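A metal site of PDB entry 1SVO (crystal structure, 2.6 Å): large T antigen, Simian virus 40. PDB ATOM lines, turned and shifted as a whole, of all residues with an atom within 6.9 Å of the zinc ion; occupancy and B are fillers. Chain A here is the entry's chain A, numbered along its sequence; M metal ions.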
ATOM      1  N   GLU A  44      27.656  25.761  19.990  1.00  0.00           N
ATOM      2  CA  GLU A  44      27.432  24.402  20.446  1.00  0.00           C
ATOM      3  C   GLU A  44      26.519  24.417  21.686  1.00  0.00           C
ATOM      4  O   GLU A  44      25.846  23.422  21.995  1.00  0.00           O
ATOM      5  CB  GLU A  44      28.754  23.739  20.786  1.00  0.00           C
ATOM      6  CG  GLU A  44      29.705  23.629  19.623  1.00  0.00           C
ATOM      7  CD  GLU A  44      30.898  22.724  19.909  1.00  0.00           C
ATOM      8  OE1 GLU A  44      31.585  22.912  20.940  1.00  0.00           O
ATOM      9  OE2 GLU A  44      31.165  21.814  19.092  1.00  0.00           O
ATOM     10  N   PHE A  45      26.497  25.571  22.365  1.00  0.00           N
ATOM     11  CA  PHE A  45      25.696  25.768  23.576  1.00  0.00           C
ATOM     12  C   PHE A  45      24.186  25.929  23.337  1.00  0.00           C
ATOM     13  O   PHE A  45      23.394  25.851  24.268  1.00  0.00           O
ATOM     14  CB  PHE A  45      26.182  26.994  24.365  1.00  0.00           C
ATOM     15  CG  PHE A  45      27.630  26.921  24.800  1.00  0.00           C
ATOM     16  CD1 PHE A  45      28.305  25.721  24.904  1.00  0.00           C
ATOM     17  CD2 PHE A  45      28.318  28.096  25.116  1.00  0.00           C
ATOM     18  CE1 PHE A  45      29.665  25.704  25.315  1.00  0.00           C
ATOM     19  CE2 PHE A  45      29.656  28.084  25.526  1.00  0.00           C
ATOM     20  CZ  PHE A  45      30.330  26.903  25.620  1.00  0.00           C
ATOM     21  N   TYR A  47      22.059  23.969  22.167  1.00  0.00           N
ATOM     22  CA  TYR A  47      21.289  22.756  22.431  1.00  0.00           C
ATOM     23  C   TYR A  47      21.129  22.537  23.943  1.00  0.00           C
ATOM     24  O   TYR A  47      22.016  22.875  24.730  1.00  0.00           O
ATOM     25  CB  TYR A  47      22.012  21.565  21.816  1.00  0.00           C
ATOM     26  CG  TYR A  47      22.369  21.790  20.371  1.00  0.00           C
ATOM     27  CD1 TYR A  47      21.383  21.872  19.397  1.00  0.00           C
ATOM     28  CD2 TYR A  47      23.702  21.917  19.982  1.00  0.00           C
ATOM     29  CE1 TYR A  47      21.721  22.073  18.069  1.00  0.00           C
ATOM     30  CE2 TYR A  47      24.053  22.116  18.660  1.00  0.00           C
ATOM     31  CZ  TYR A  47      23.064  22.189  17.708  1.00  0.00           C
ATOM     32  OH  TYR A  47      23.448  22.352  16.401  1.00  0.00           O
ATOM     33  N   SER A  48      20.000  21.956  24.341  1.00  0.00           N
ATOM     34  CA  SER A  48      19.784  21.724  25.756  1.00  0.00           C
ATOM     35  C   SER A  48      20.985  20.958  26.296  1.00  0.00           C
ATOM     36  O   SER A  48      21.478  20.023  25.674  1.00  0.00           O
ATOM     37  CB  SER A  48      18.507  20.921  25.999  1.00  0.00           C
ATOM     38  OG  SER A  48      18.762  19.529  25.971  1.00  0.00           O
ATOM     39  N   PHE A  49      21.454  21.405  27.446  1.00  0.00           N
ATOM     40  CA  PHE A  49      22.585  20.788  28.112  1.00  0.00           C
ATOM     41  C   PHE A  49      22.019  19.614  28.890  1.00  0.00           C
ATOM     42  O   PHE A  49      22.742  18.709  29.294  1.00  0.00           O
ATOM     43  CB  PHE A  49      23.254  21.811  29.030  1.00  0.00           C
ATOM     44  CG  PHE A  49      23.145  21.479  30.480  1.00  0.00           C
ATOM     45  CD1 PHE A  49      24.146  20.763  31.122  1.00  0.00           C
ATOM     46  CD2 PHE A  49      22.035  21.891  31.226  1.00  0.00           C
ATOM     47  CE1 PHE A  49      24.052  20.467  32.491  1.00  0.00           C
ATOM     48  CE2 PHE A  49      21.929  21.597  32.590  1.00  0.00           C
ATOM     49  CZ  PHE A  49      22.938  20.880  33.227  1.00  0.00           C
ATOM     50  N   CYS A  52      23.249  17.077  26.621  1.00  0.00           N
ATOM     51  CA  CYS A  52      24.569  17.219  25.997  1.00  0.00           C
ATOM     52  C   CYS A  52      25.529  16.074  26.318  1.00  0.00           C
ATOM     53  O   CYS A  52      25.899  15.857  27.468  1.00  0.00           O
ATOM     54  CB  CYS A  52      25.185  18.583  26.420  1.00  0.00           C
ATOM     55  SG  CYS A  52      26.997  18.820  26.209  1.00  0.00           S
ATOM     56  N   LEU A  53      25.912  15.320  25.294  1.00  0.00           N
ATOM     57  CA  LEU A  53      26.843  14.227  25.499  1.00  0.00           C
ATOM     58  C   LEU A  53      28.267  14.750  25.636  1.00  0.00           C
ATOM     59  O   LEU A  53      29.113  14.103  26.250  1.00  0.00           O
ATOM     60  CB  LEU A  53      26.773  13.227  24.343  1.00  0.00           C
ATOM     61  CG  LEU A  53      25.927  11.957  24.562  1.00  0.00           C
ATOM     62  CD1 LEU A  53      25.889  11.120  23.280  1.00  0.00           C
ATOM     63  CD2 LEU A  53      26.517  11.140  25.726  1.00  0.00           C
ATOM     64  N   LYS A  54      28.526  15.915  25.047  1.00  0.00           N
ATOM     65  CA  LYS A  54      29.849  16.535  25.090  1.00  0.00           C
ATOM     66  C   LYS A  54      30.178  16.874  26.525  1.00  0.00           C
ATOM     67  O   LYS A  54      31.341  16.823  26.933  1.00  0.00           O
ATOM     68  CB  LYS A  54      29.859  17.810  24.244  1.00  0.00           C
ATOM     69  CG  LYS A  54      29.485  17.550  22.799  1.00  0.00           C
ATOM     70  CD  LYS A  54      29.816  18.711  21.872  1.00  0.00           C
ATOM     71  CE  LYS A  54      29.615  18.277  20.420  1.00  0.00           C
ATOM     72  NZ  LYS A  54      29.801  19.382  19.444  1.00  0.00           N
ATOM     73  N   CYS A  55      29.147  17.222  27.277  1.00  0.00           N
ATOM     74  CA  CYS A  55      29.253  17.571  28.679  1.00  0.00           C
ATOM     75  C   CYS A  55      29.314  16.282  29.494  1.00  0.00           C
ATOM     76  O   CYS A  55      30.274  16.066  30.244  1.00  0.00           O
ATOM     77  CB  CYS A  55      28.027  18.371  29.090  1.00  0.00           C
ATOM     78  SG  CYS A  55      27.653  19.728  27.945  1.00  0.00           S
ATOM     79  N   ILE A  56      28.296  15.439  29.360  1.00  0.00           N
ATOM     80  CA  ILE A  56      28.257  14.166  30.067  1.00  0.00           C
ATOM     81  C   ILE A  56      29.603  13.443  29.913  1.00  0.00           C
ATOM     82  O   ILE A  56      30.190  12.957  30.899  1.00  0.00           O
ATOM     83  CB  ILE A  56      27.100  13.245  29.532  1.00  0.00           C
ATOM     84  CG1 ILE A  56      25.740  13.884  29.840  1.00  0.00           C
ATOM     85  CG2 ILE A  56      27.166  11.859  30.176  1.00  0.00           C
ATOM     86  CD1 ILE A  56      24.551  13.111  29.293  1.00  0.00           C
ATOM     87  N   HIS A  63      34.061  23.578  26.763  1.00  0.00           N
ATOM     88  CA  HIS A  63      32.659  23.371  26.458  1.00  0.00           C
ATOM     89  C   HIS A  63      31.818  22.955  27.678  1.00  0.00           C
ATOM     90  O   HIS A  63      30.842  23.616  28.038  1.00  0.00           O
ATOM     91  CB  HIS A  63      32.545  22.301  25.384  1.00  0.00           C
ATOM     92  CG  HIS A  63      31.128  22.013  24.982  1.00  0.00           C
ATOM     93  ND1 HIS A  63      30.404  22.876  24.195  1.00  0.00           N
ATOM     94  CD2 HIS A  63      30.321  20.971  25.260  1.00  0.00           C
ATOM     95  CE1 HIS A  63      29.201  22.371  23.995  1.00  0.00           C
ATOM     96  NE2 HIS A  63      29.119  21.216  24.628  1.00  0.00           N
ATOM     97  N   TYR A  64      32.211  21.853  28.303  1.00  0.00           N
ATOM     98  CA  TYR A  64      31.442  21.359  29.421  1.00  0.00           C
ATOM     99  C   TYR A  64      31.459  22.179  30.712  1.00  0.00           C
ATOM    100  O   TYR A  64      30.764  21.839  31.653  1.00  0.00           O
ATOM    101  CB  TYR A  64      31.837  19.900  29.711  1.00  0.00           C
ATOM    102  CG  TYR A  64      33.219  19.701  30.278  1.00  0.00           C
ATOM    103  CD1 TYR A  64      33.527  20.132  31.574  1.00  0.00           C
ATOM    104  CD2 TYR A  64      34.213  19.037  29.560  1.00  0.00           C
ATOM    105  CE1 TYR A  64      34.787  19.915  32.149  1.00  0.00           C
ATOM    106  CE2 TYR A  64      35.498  18.805  30.123  1.00  0.00           C
ATOM    107  CZ  TYR A  64      35.771  19.242  31.413  1.00  0.00           C
ATOM    108  OH  TYR A  64      37.009  19.060  32.000  1.00  0.00           O
ATOM    109  N   TYR A  66      30.942  25.546  30.517  1.00  0.00           N
ATOM    110  CA  TYR A  66      30.166  26.739  30.216  1.00  0.00           C
ATOM    111  C   TYR A  66      28.832  26.458  29.571  1.00  0.00           C
ATOM    112  O   TYR A  66      27.964  27.332  29.579  1.00  0.00           O
ATOM    113  CB  TYR A  66      30.980  27.669  29.329  1.00  0.00           C
ATOM    114  CG  TYR A  66      32.335  28.015  29.891  1.00  0.00           C
ATOM    115  CD1 TYR A  66      33.422  27.147  29.745  1.00  0.00           C
ATOM    116  CD2 TYR A  66      32.529  29.211  30.587  1.00  0.00           C
ATOM    117  CE1 TYR A  66      34.682  27.468  30.281  1.00  0.00           C
ATOM    118  CE2 TYR A  66      33.785  29.534  31.137  1.00  0.00           C
ATOM    119  CZ  TYR A  66      34.856  28.659  30.986  1.00  0.00           C
ATOM    120  OH  TYR A  66      36.077  28.968  31.539  1.00  0.00           O
ATOM    121  N   HIS A  67      28.646  25.265  29.014  1.00  0.00           N
ATOM    122  CA  HIS A  67      27.380  24.950  28.338  1.00  0.00           C
ATOM    123  C   HIS A  67      26.164  25.295  29.202  1.00  0.00           C
ATOM    124  O   HIS A  67      25.236  25.962  28.745  1.00  0.00           O
ATOM    125  CB  HIS A  67      27.303  23.476  27.904  1.00  0.00           C
ATOM    126  CG  HIS A  67      26.126  23.158  27.004  1.00  0.00           C
ATOM    127  ND1 HIS A  67      25.887  21.895  26.509  1.00  0.00           N
ATOM    128  CD2 HIS A  67      25.151  23.955  26.508  1.00  0.00           C
ATOM    129  CE1 HIS A  67      24.815  21.918  25.744  1.00  0.00           C
ATOM    130  NE2 HIS A  67      24.348  23.154  25.715  1.00  0.00           N
ATOM    131  N   GLU A  68      26.190  24.819  30.445  1.00  0.00           N
ATOM    132  CA  GLU A  68      25.117  25.069  31.395  1.00  0.00           C
ATOM    133  C   GLU A  68      24.788  26.566  31.461  1.00  0.00           C
ATOM    134  O   GLU A  68      23.723  27.005  30.998  1.00  0.00           O
ATOM    135  CB  GLU A  68      25.562  24.591  32.782  1.00  0.00           C
ATOM    136  CG  GLU A  68      24.601  23.621  33.481  1.00  0.00           C
ATOM    137  CD  GLU A  68      23.260  24.258  33.858  1.00  0.00           C
ATOM    138  OE1 GLU A  68      22.538  23.666  34.700  1.00  0.00           O
ATOM    139  OE2 GLU A  68      22.926  25.331  33.303  1.00  0.00           O
HETATM  140 ZN    ZN M   1      27.591  20.766  26.244  1.00  0.00          ZN
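Of the 15 residues printed, 4 come within 4 Å of the zinc ion.
The zinc ion is bound by SG of Cys 55, SG of Cys 52, ND1 of His 67 and NE2 of His 63.
The side-chain sulfur (SG) of Cys 55 is disulfide-bonded to the side-chain sulfur (SG) of Cys 52 (2.1 Å). SG of Cys 52 sits close to N of Lys 54 (3.5 Å). NE2 of His 67 is in hydrogen-bond range of O of Phe 45 (3.2 Å). NE2 of His 67 sits at hydrogen-bond distance from O of Tyr 47 (2.5 Å). The side-chain carboxylate (OE1) of Glu 44 lies within hydrogen-bond range of a ring nitrogen (ND1) of His 63 (3.5 Å).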
